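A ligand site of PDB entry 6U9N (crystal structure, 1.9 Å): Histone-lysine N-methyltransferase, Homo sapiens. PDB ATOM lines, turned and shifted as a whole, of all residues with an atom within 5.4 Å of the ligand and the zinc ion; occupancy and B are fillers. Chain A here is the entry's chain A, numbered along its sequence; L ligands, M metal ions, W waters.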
ATOM      1  N   ILE A  27       4.012  12.384 -12.946  1.00  0.00           N
ATOM      2  CA  ILE A  27       4.087  13.842 -12.961  1.00  0.00           C
ATOM      3  C   ILE A  27       2.795  14.376 -13.601  1.00  0.00           C
ATOM      4  O   ILE A  27       2.060  15.118 -12.933  1.00  0.00           O
ATOM      5  CB  ILE A  27       5.376  14.383 -13.652  1.00  0.00           C
ATOM      6  CG1 ILE A  27       6.646  14.006 -12.845  1.00  0.00           C
ATOM      7  CG2 ILE A  27       5.292  15.907 -13.845  1.00  0.00           C
ATOM      8  CD1 ILE A  27       8.013  14.164 -13.642  1.00  0.00           C
ATOM      9  N   HIS A  28       2.483  13.971 -14.853  1.00  0.00           N
ATOM     10  CA  HIS A  28       1.256  14.340 -15.566  1.00  0.00           C
ATOM     11  C   HIS A  28       1.093  13.481 -16.813  1.00  0.00           C
ATOM     12  O   HIS A  28       2.066  13.321 -17.561  1.00  0.00           O
ATOM     13  CB  HIS A  28       1.311  15.830 -15.990  1.00  0.00           C
ATOM     14  CG  HIS A  28       0.157  16.281 -16.841  1.00  0.00           C
ATOM     15  ND1 HIS A  28       0.178  16.144 -18.223  1.00  0.00           N
ATOM     16  CD2 HIS A  28      -0.967  16.950 -16.483  1.00  0.00           C
ATOM     17  CE1 HIS A  28      -0.949  16.683 -18.667  1.00  0.00           C
ATOM     18  NE2 HIS A  28      -1.651  17.226 -17.660  1.00  0.00           N
ATOM     19  N   GLY A  29      -0.145  13.039 -17.063  1.00  0.00           N
ATOM     20  CA  GLY A  29      -0.567  12.312 -18.277  1.00  0.00           C
ATOM     21  C   GLY A  29       0.418  11.256 -18.736  1.00  0.00           C
ATOM     22  O   GLY A  29       0.672  10.307 -18.000  1.00  0.00           O
ATOM     23  N   ARG A  30       0.996  11.454 -19.936  1.00  0.00           N
ATOM     24  CA  ARG A  30       2.046  10.566 -20.445  1.00  0.00           C
ATOM     25  C   ARG A  30       3.339  11.351 -20.429  1.00  0.00           C
ATOM     26  O   ARG A  30       3.330  12.582 -20.497  1.00  0.00           O
ATOM     27  CB  ARG A  30       1.750  10.025 -21.875  1.00  0.00           C
ATOM     28  CG  ARG A  30       0.584   9.020 -21.910  1.00  0.00           C
ATOM     29  CD  ARG A  30       0.285   8.542 -23.323  1.00  0.00           C
ATOM     30  NE  ARG A  30      -0.290   9.625 -24.127  1.00  0.00           N
ATOM     31  CZ  ARG A  30      -0.533   9.538 -25.429  1.00  0.00           C
ATOM     32  NH1 ARG A  30      -0.223   8.443 -26.103  1.00  0.00           N
ATOM     33  NH2 ARG A  30      -1.086  10.562 -26.075  1.00  0.00           N
ATOM     34  N   GLY A  31       4.443  10.625 -20.306  1.00  0.00           N
ATOM     35  CA  GLY A  31       5.773  11.230 -20.307  1.00  0.00           C
ATOM     36  C   GLY A  31       6.722  10.417 -21.138  1.00  0.00           C
ATOM     37  O   GLY A  31       6.388   9.311 -21.572  1.00  0.00           O
ATOM     38  N   GLY A  70      -5.230  17.457 -28.725  1.00  0.00           N
ATOM     39  CA  GLY A  70      -4.239  17.972 -27.768  1.00  0.00           C
ATOM     40  C   GLY A  70      -3.241  18.855 -28.498  1.00  0.00           C
ATOM     41  O   GLY A  70      -2.773  18.482 -29.574  1.00  0.00           O
ATOM     42  N   CYS A  71      -2.982  20.053 -27.972  1.00  0.00           N
ATOM     43  CA  CYS A  71      -2.069  21.039 -28.581  1.00  0.00           C
ATOM     44  C   CYS A  71      -0.700  20.891 -27.941  1.00  0.00           C
ATOM     45  O   CYS A  71      -0.607  20.938 -26.720  1.00  0.00           O
ATOM     46  CB  CYS A  71      -2.629  22.453 -28.382  1.00  0.00           C
ATOM     47  SG  CYS A  71      -1.537  23.760 -29.022  1.00  0.00           S
ATOM     48  N   TYR A  72       0.343  20.628 -28.741  1.00  0.00           N
ATOM     49  CA  TYR A  72       1.719  20.393 -28.270  1.00  0.00           C
ATOM     50  C   TYR A  72       2.593  21.415 -28.947  1.00  0.00           C
ATOM     51  O   TYR A  72       2.819  21.338 -30.157  1.00  0.00           O
ATOM     52  CB  TYR A  72       2.199  18.977 -28.679  1.00  0.00           C
ATOM     53  CG  TYR A  72       1.477  17.861 -27.947  1.00  0.00           C
ATOM     54  CD1 TYR A  72       1.984  17.337 -26.764  1.00  0.00           C
ATOM     55  CD2 TYR A  72       0.243  17.397 -28.385  1.00  0.00           C
ATOM     56  CE1 TYR A  72       1.291  16.374 -26.032  1.00  0.00           C
ATOM     57  CE2 TYR A  72      -0.469  16.425 -27.660  1.00  0.00           C
ATOM     58  CZ  TYR A  72       0.063  15.925 -26.480  1.00  0.00           C
ATOM     59  OH  TYR A  72      -0.576  14.962 -25.753  1.00  0.00           O
ATOM     60  N   ARG A  92       7.381  15.367 -27.703  1.00  0.00           N
ATOM     61  CA  ARG A  92       6.308  16.275 -27.298  1.00  0.00           C
ATOM     62  C   ARG A  92       5.703  15.905 -25.931  1.00  0.00           C
ATOM     63  O   ARG A  92       4.980  16.711 -25.351  1.00  0.00           O
ATOM     64  CB  ARG A  92       5.238  16.409 -28.401  1.00  0.00           C
ATOM     65  CG  ARG A  92       4.281  15.250 -28.552  1.00  0.00           C
ATOM     66  CD  ARG A  92       3.523  15.414 -29.872  1.00  0.00           C
ATOM     67  NE  ARG A  92       2.448  14.427 -30.031  1.00  0.00           N
ATOM     68  CZ  ARG A  92       2.610  13.202 -30.514  1.00  0.00           C
ATOM     69  NH1 ARG A  92       3.810  12.777 -30.877  1.00  0.00           N
ATOM     70  NH2 ARG A  92       1.569  12.396 -30.648  1.00  0.00           N
ATOM     71  N   PHE A  93       5.955  14.674 -25.452  1.00  0.00           N
ATOM     72  CA  PHE A  93       5.401  14.229 -24.148  1.00  0.00           C
ATOM     73  C   PHE A  93       6.352  14.526 -22.987  1.00  0.00           C
ATOM     74  O   PHE A  93       6.005  14.188 -21.867  1.00  0.00           O
ATOM     75  CB  PHE A  93       5.112  12.724 -24.210  1.00  0.00           C
ATOM     76  CG  PHE A  93       4.006  12.404 -25.179  1.00  0.00           C
ATOM     77  CD1 PHE A  93       2.675  12.638 -24.845  1.00  0.00           C
ATOM     78  CD2 PHE A  93       4.291  11.918 -26.452  1.00  0.00           C
ATOM     79  CE1 PHE A  93       1.651  12.380 -25.761  1.00  0.00           C
ATOM     80  CE2 PHE A  93       3.262  11.666 -27.362  1.00  0.00           C
ATOM     81  CZ  PHE A  93       1.952  11.894 -27.005  1.00  0.00           C
ATOM     82  N   ILE A  94       7.532  15.146 -23.240  1.00  0.00           N
ATOM     83  CA  ILE A  94       8.495  15.436 -22.161  1.00  0.00           C
ATOM     84  C   ILE A  94       7.867  16.432 -21.189  1.00  0.00           C
ATOM     85  O   ILE A  94       7.515  17.542 -21.610  1.00  0.00           O
ATOM     86  CB  ILE A  94       9.905  15.934 -22.644  1.00  0.00           C
ATOM     87  CG1 ILE A  94      10.602  14.934 -23.556  1.00  0.00           C
ATOM     88  CG2 ILE A  94      10.822  16.222 -21.404  1.00  0.00           C
ATOM     89  CD1 ILE A  94      11.671  15.543 -24.444  1.00  0.00           C
ATOM     90  N   ASN A  95       7.765  16.033 -19.906  1.00  0.00           N
ATOM     91  CA  ASN A  95       7.219  16.844 -18.812  1.00  0.00           C
ATOM     92  C   ASN A  95       8.250  17.758 -18.190  1.00  0.00           C
ATOM     93  O   ASN A  95       9.443  17.524 -18.342  1.00  0.00           O
ATOM     94  CB  ASN A  95       6.604  15.928 -17.705  1.00  0.00           C
ATOM     95  CG  ASN A  95       5.249  15.382 -18.076  1.00  0.00           C
ATOM     96  OD1 ASN A  95       4.406  16.077 -18.659  1.00  0.00           O
ATOM     97  ND2 ASN A  95       4.987  14.125 -17.761  1.00  0.00           N
ATOM     98  N   HIS A  96       7.797  18.806 -17.471  1.00  0.00           N
ATOM     99  CA  HIS A  96       8.657  19.750 -16.741  1.00  0.00           C
ATOM    100  C   HIS A  96       9.137  19.127 -15.414  1.00  0.00           C
ATOM    101  O   HIS A  96       8.408  18.334 -14.816  1.00  0.00           O
ATOM    102  CB  HIS A  96       7.884  21.045 -16.399  1.00  0.00           C
ATOM    103  CG  HIS A  96       8.587  21.925 -15.405  1.00  0.00           C
ATOM    104  ND1 HIS A  96       9.633  22.753 -15.780  1.00  0.00           N
ATOM    105  CD2 HIS A  96       8.403  22.026 -14.071  1.00  0.00           C
ATOM    106  CE1 HIS A  96      10.049  23.328 -14.664  1.00  0.00           C
ATOM    107  NE2 HIS A  96       9.342  22.926 -13.608  1.00  0.00           N
ATOM    108  N   SER A  97      10.342  19.543 -14.935  1.00  0.00           N
ATOM    109  CA  SER A  97      10.880  19.212 -13.609  1.00  0.00           C
ATOM    110  C   SER A  97      11.826  20.287 -13.186  1.00  0.00           C
ATOM    111  O   SER A  97      12.566  20.812 -14.011  1.00  0.00           O
ATOM    112  CB  SER A  97      11.586  17.862 -13.574  1.00  0.00           C
ATOM    113  OG  SER A  97      12.211  17.624 -12.320  1.00  0.00           O
ATOM    114  N   CYS A  98      11.822  20.588 -11.873  1.00  0.00           N
ATOM    115  CA  CYS A  98      12.632  21.596 -11.215  1.00  0.00           C
ATOM    116  C   CYS A  98      14.033  21.067 -10.903  1.00  0.00           C
ATOM    117  O   CYS A  98      14.928  21.835 -10.555  1.00  0.00           O
ATOM    118  CB  CYS A  98      11.933  22.123  -9.977  1.00  0.00           C
ATOM    119  SG  CYS A  98      10.247  22.706 -10.298  1.00  0.00           S
ATOM    120  N   TYR A 133      10.852  23.890 -18.073  1.00  0.00           N
ATOM    121  CA  TYR A 133      10.049  24.631 -19.063  1.00  0.00           C
ATOM    122  C   TYR A 133      10.392  26.117 -18.954  1.00  0.00           C
ATOM    123  O   TYR A 133      10.612  26.615 -17.854  1.00  0.00           O
ATOM    124  CB  TYR A 133       8.541  24.444 -18.792  1.00  0.00           C
ATOM    125  CG  TYR A 133       7.930  23.148 -19.293  1.00  0.00           C
ATOM    126  CD1 TYR A 133       8.713  22.071 -19.682  1.00  0.00           C
ATOM    127  CD2 TYR A 133       6.539  22.988 -19.330  1.00  0.00           C
ATOM    128  CE1 TYR A 133       8.151  20.885 -20.139  1.00  0.00           C
ATOM    129  CE2 TYR A 133       5.968  21.798 -19.758  1.00  0.00           C
ATOM    130  CZ  TYR A 133       6.774  20.738 -20.146  1.00  0.00           C
ATOM    131  OH  TYR A 133       6.200  19.575 -20.555  1.00  0.00           O
ATOM    132  N   PRO A 145       0.470  24.651 -11.045  1.00  0.00           N
ATOM    133  CA  PRO A 145       1.222  23.914 -10.004  1.00  0.00           C
ATOM    134  C   PRO A 145       2.120  22.821 -10.578  1.00  0.00           C
ATOM    135  O   PRO A 145       1.764  22.186 -11.569  1.00  0.00           O
ATOM    136  CB  PRO A 145       0.125  23.329  -9.098  1.00  0.00           C
ATOM    137  CG  PRO A 145      -1.120  23.361  -9.912  1.00  0.00           C
ATOM    138  CD  PRO A 145      -0.988  24.490 -10.876  1.00  0.00           C
ATOM    139  N   CYS A 146       3.325  22.652 -10.001  1.00  0.00           N
ATOM    140  CA  CYS A 146       4.294  21.667 -10.478  1.00  0.00           C
ATOM    141  C   CYS A 146       4.253  20.359  -9.687  1.00  0.00           C
ATOM    142  O   CYS A 146       4.213  20.383  -8.453  1.00  0.00           O
ATOM    143  CB  CYS A 146       5.701  22.252 -10.480  1.00  0.00           C
ATOM    144  SG  CYS A 146       6.970  21.070 -10.924  1.00  0.00           S
ATOM    145  N   ASN A 147       4.346  19.228 -10.403  1.00  0.00           N
ATOM    146  CA  ASN A 147       4.297  17.872  -9.847  1.00  0.00           C
ATOM    147  C   ASN A 147       5.579  17.066 -10.038  1.00  0.00           C
ATOM    148  O   ASN A 147       5.554  15.842  -9.924  1.00  0.00           O
ATOM    149  CB  ASN A 147       3.082  17.117 -10.387  1.00  0.00           C
ATOM    150  CG  ASN A 147       2.606  15.997  -9.499  1.00  0.00           C
ATOM    151  OD1 ASN A 147       2.400  16.153  -8.288  1.00  0.00           O
ATOM    152  ND2 ASN A 147       2.428  14.826 -10.085  1.00  0.00           N
ATOM    153  N   CYS A 148       6.725  17.732 -10.283  1.00  0.00           N
ATOM    154  CA  CYS A 148       7.961  16.961 -10.449  1.00  0.00           C
ATOM    155  C   CYS A 148       8.332  16.160  -9.196  1.00  0.00           C
ATOM    156  O   CYS A 148       8.921  15.094  -9.328  1.00  0.00           O
ATOM    157  CB  CYS A 148       9.116  17.844 -10.921  1.00  0.00           C
ATOM    158  SG  CYS A 148       9.772  18.964  -9.668  1.00  0.00           S
ATOM    159  N   GLY A 149       7.969  16.702  -8.025  1.00  0.00           N
ATOM    160  CA  GLY A 149       8.182  16.085  -6.709  1.00  0.00           C
ATOM    161  C   GLY A 149       9.580  16.218  -6.164  1.00  0.00           C
ATOM    162  O   GLY A 149       9.913  15.566  -5.173  1.00  0.00           O
ATOM    163  N   ALA A 150      10.431  17.063  -6.796  1.00  0.00           N
ATOM    164  CA  ALA A 150      11.825  17.276  -6.385  1.00  0.00           C
ATOM    165  C   ALA A 150      11.920  17.941  -5.015  1.00  0.00           C
ATOM    166  O   ALA A 150      10.971  18.604  -4.589  1.00  0.00           O
ATOM    167  CB  ALA A 150      12.565  18.088  -7.433  1.00  0.00           C
ATOM    168  N   CYS A 153      11.799  21.851  -5.432  1.00  0.00           N
ATOM    169  CA  CYS A 153      10.708  22.198  -6.340  1.00  0.00           C
ATOM    170  C   CYS A 153      10.326  23.667  -6.232  1.00  0.00           C
ATOM    171  O   CYS A 153      10.179  24.173  -5.128  1.00  0.00           O
ATOM    172  CB  CYS A 153       9.507  21.285  -6.120  1.00  0.00           C
ATOM    173  SG  CYS A 153       8.169  21.533  -7.326  1.00  0.00           S
ATOM    174  N   ARG A 154      10.126  24.345  -7.386  1.00  0.00           N
ATOM    175  CA  ARG A 154       9.699  25.751  -7.480  1.00  0.00           C
ATOM    176  C   ARG A 154       8.171  25.836  -7.254  1.00  0.00           C
ATOM    177  O   ARG A 154       7.612  26.936  -7.164  1.00  0.00           O
ATOM    178  CB  ARG A 154      10.069  26.358  -8.853  1.00  0.00           C
ATOM    179  CG  ARG A 154      11.549  26.237  -9.245  1.00  0.00           C
ATOM    180  CD  ARG A 154      11.935  27.125 -10.411  1.00  0.00           C
ATOM    181  NE  ARG A 154      11.544  26.558 -11.711  1.00  0.00           N
ATOM    182  CZ  ARG A 154      10.446  26.902 -12.377  1.00  0.00           C
ATOM    183  NH1 ARG A 154      10.172  26.353 -13.552  1.00  0.00           N
ATOM    184  NH2 ARG A 154       9.600  27.799 -11.875  1.00  0.00           N
ATOM    185  N   LYS A 155       7.497  24.665  -7.197  1.00  0.00           N
ATOM    186  CA  LYS A 155       6.072  24.440  -6.968  1.00  0.00           C
ATOM    187  C   LYS A 155       5.154  24.991  -8.072  1.00  0.00           C
ATOM    188  O   LYS A 155       3.935  24.710  -8.045  1.00  0.00           O
ATOM    189  CB  LYS A 155       5.644  24.915  -5.571  1.00  0.00           C
ATOM    190  CG  LYS A 155       6.531  24.343  -4.422  1.00  0.00           C
ATOM    191  CD  LYS A 155       6.252  22.870  -4.100  1.00  0.00           C
ATOM    192  CE  LYS A 155       7.101  22.373  -2.959  1.00  0.00           C
ATOM    193  NZ  LYS A 155       6.802  20.960  -2.615  1.00  0.00           N
HETATM  194  O1  LIG L   1       0.237  15.250 -23.143  1.00  0.00           O
HETATM  195  C1  LIG L   1       0.762  14.929 -22.083  1.00  0.00           C
HETATM  196  O2  LIG L   1       0.498  13.735 -21.538  1.00  0.00           O
HETATM  197  C2  LIG L   1       1.736  15.743 -21.244  1.00  0.00           C
HETATM  198  N1  LIG L   1       2.142  15.095 -19.985  1.00  0.00           N
HETATM  199  C3  LIG L   1       2.981  16.013 -22.106  1.00  0.00           C
HETATM  200  C4  LIG L   1       3.485  17.457 -21.857  1.00  0.00           C
HETATM  201  N2  LIG L   1       2.480  18.551 -22.074  1.00  0.00           N
HETATM  202  C5  LIG L   1       2.803  19.875 -21.410  1.00  0.00           C
HETATM  203  C6  LIG L   1       1.807  20.011 -20.247  1.00  0.00           C
HETATM  204  C7  LIG L   1       2.041  21.339 -19.481  1.00  0.00           C
HETATM  205  O3  LIG L   1       1.393  22.427 -20.072  1.00  0.00           O
HETATM  206  C8  LIG L   1       1.341  20.983 -18.156  1.00  0.00           C
HETATM  207  O4  LIG L   1      -0.021  21.032 -18.281  1.00  0.00           O
HETATM  208  O5  LIG L   1       1.976  18.966 -19.305  1.00  0.00           O
HETATM  209  C9  LIG L   1       1.700  19.438 -18.027  1.00  0.00           C
HETATM  210  N3  LIG L   1       2.880  19.226 -17.164  1.00  0.00           N
HETATM  211  C10 LIG L   1       2.950  19.287 -15.780  1.00  0.00           C
HETATM  212  N4  LIG L   1       1.958  19.454 -14.841  1.00  0.00           N
HETATM  213  C11 LIG L   1       2.445  19.500 -13.594  1.00  0.00           C
HETATM  214  N5  LIG L   1       3.745  19.409 -13.166  1.00  0.00           N
HETATM  215  C12 LIG L   1       4.212  19.014 -17.618  1.00  0.00           C
HETATM  216  N6  LIG L   1       5.097  18.953 -16.642  1.00  0.00           N
HETATM  217  C13 LIG L   1       4.333  19.143 -15.476  1.00  0.00           C
HETATM  218  C14 LIG L   1       4.704  19.240 -14.111  1.00  0.00           C
HETATM  219  N7  LIG L   1       6.005  19.151 -13.718  1.00  0.00           N
HETATM  220  C15 LIG L   1       1.824  18.648 -23.408  1.00  0.00           C
HETATM  221  C16 LIG L   1       0.441  19.350 -23.307  1.00  0.00           C
HETATM  222  C17 LIG L   1      -0.563  19.089 -24.466  1.00  0.00           C
HETATM  223  N8  LIG L   1      -1.147  17.934 -23.665  1.00  0.00           N
HETATM  224  C18 LIG L   1      -0.645  18.633 -22.440  1.00  0.00           C
HETATM  225  C19 LIG L   1      -2.638  17.777 -23.803  1.00  0.00           C
HETATM  226  C20 LIG L   1      -3.167  17.021 -22.607  1.00  0.00           C
HETATM  227  C21 LIG L   1      -2.869  15.654 -22.461  1.00  0.00           C
HETATM  228  C22 LIG L   1      -3.296  14.955 -21.305  1.00  0.00           C
HETATM  229  C23 LIG L   1      -4.026  15.647 -20.322  1.00  0.00           C
HETATM  230 CL1  LIG L   1      -4.498  14.787 -18.860  1.00  0.00          CL
HETATM  231  C24 LIG L   1      -4.360  17.002 -20.452  1.00  0.00           C
HETATM  232  C25 LIG L   1      -3.920  17.695 -21.609  1.00  0.00           C
HETATM  233 ZN    ZN M   1       8.888  21.053  -9.642  1.00  0.00          ZN
HETATM  234  O   HOH W   1      -3.922  19.146 -17.741  1.00  0.00           O
HETATM  235  O   HOH W   2      -1.252  12.248 -22.773  1.00  0.00           O
HETATM  236  O   HOH W   3      -0.437  20.678 -15.485  1.00  0.00           O
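CG2 of Ile 27 touches N7 of the ligand (3.3 Å). Gly 29 touches the ligand (CA to O2, 3.7 Å). Cys 71 touches the ligand (O to C17, 2.9 Å). O of Arg 92 touches C4 of the ligand (3.9 Å). Phe 93 touches the ligand. Tyr 133 touches the ligand (OH to C5, 3.5 Å). O of Pro 145 touches C11 of the ligand, 3.4 Å away. Hydrophobic or aromatic side chains that line the ligand: Ile 27, His 28, Tyr 72, Phe 93, His 96 and Tyr 133. Within 4 Å of the ligand: Ile 27, His 28, Gly 29, Arg 30, Cys 71, Tyr 72, Arg 92, Phe 93, Asn 95, His 96, Tyr 133, Pro 145, Cys 146, Asn 147 and Cys 148.
The side-chain sulfur (SG) of Cys 98 lies close to a ring nitrogen (NE2) of His 96 (3.4 Å). The backbone NH of Arg 154 sits close to the side-chain sulfur of Cys 98 (3.3 Å). The backbone NH (N) of Ala 150 lies close to the side-chain sulfur (SG) of Cys 148 (3.5 Å). N of Cys 146 sits at hydrogen-bond distance from O of Lys 155. The backbone NH (N) of Lys 155 lies close to the side-chain sulfur (SG) of Cys 153 (3.2 Å). ND1 of His 96 sits at hydrogen-bond distance from N of Tyr 133. The backbone carbonyl oxygen (O) of His 28 sits at hydrogen-bond distance from the side-chain amide nitrogen (ND2) of Asn 95, 3.0 Å away. OH of Tyr 133 lies within hydrogen-bond range of O of Ile 94.
Water W2 bridges an oxygen (O2) of the ligand and the guanidinium group (NE) of Arg 30.
The zinc ion is bound by the side-chain sulfur of Cys 98, the side-chain sulfur of Cys 148, the side-chain sulfur of Cys 146 and the side-chain sulfur of Cys 153.
N7 of the ligand lies close to SG of Cys 146 (3.5 Å). OH of Tyr 72 lies within hydrogen-bond range of O1 of the ligand (2.7 Å). The backbone NH (N) of His 96 sits at hydrogen-bond distance from a nitrogen (N6) of the ligand. A nitrogen (N7) of the ligand lies within hydrogen-bond range of the backbone carbonyl oxygen (O) of His 96, at 2.8 Å. N1 of the ligand lies within hydrogen-bond range of OD1 of Asn 95, at 2.8 Å. An oxygen (O2) of the ligand lies within hydrogen-bond range of the backbone NH (N) of Arg 30, at 2.8 Å. The backbone carbonyl oxygen (O) of Arg 30 is in hydrogen-bond range of a nitrogen (N1) of the ligand, 2.8 Å away. N of Asn 147 lies within hydrogen-bond range of N5 of the ligand (2.8 Å). The backbone carbonyl oxygen (O) of His 28 lies within hydrogen-bond range of a nitrogen (N1) of the ligand, 3.0 Å away. ND1 of His 28 sits at hydrogen-bond distance from N1 of the ligand (2.8 Å).
Of the 25 residues printed, 4 come within 4 Å of the zinc ion. Along chain A the residues within 4 Å of the zinc ion span positions 98 to 153.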
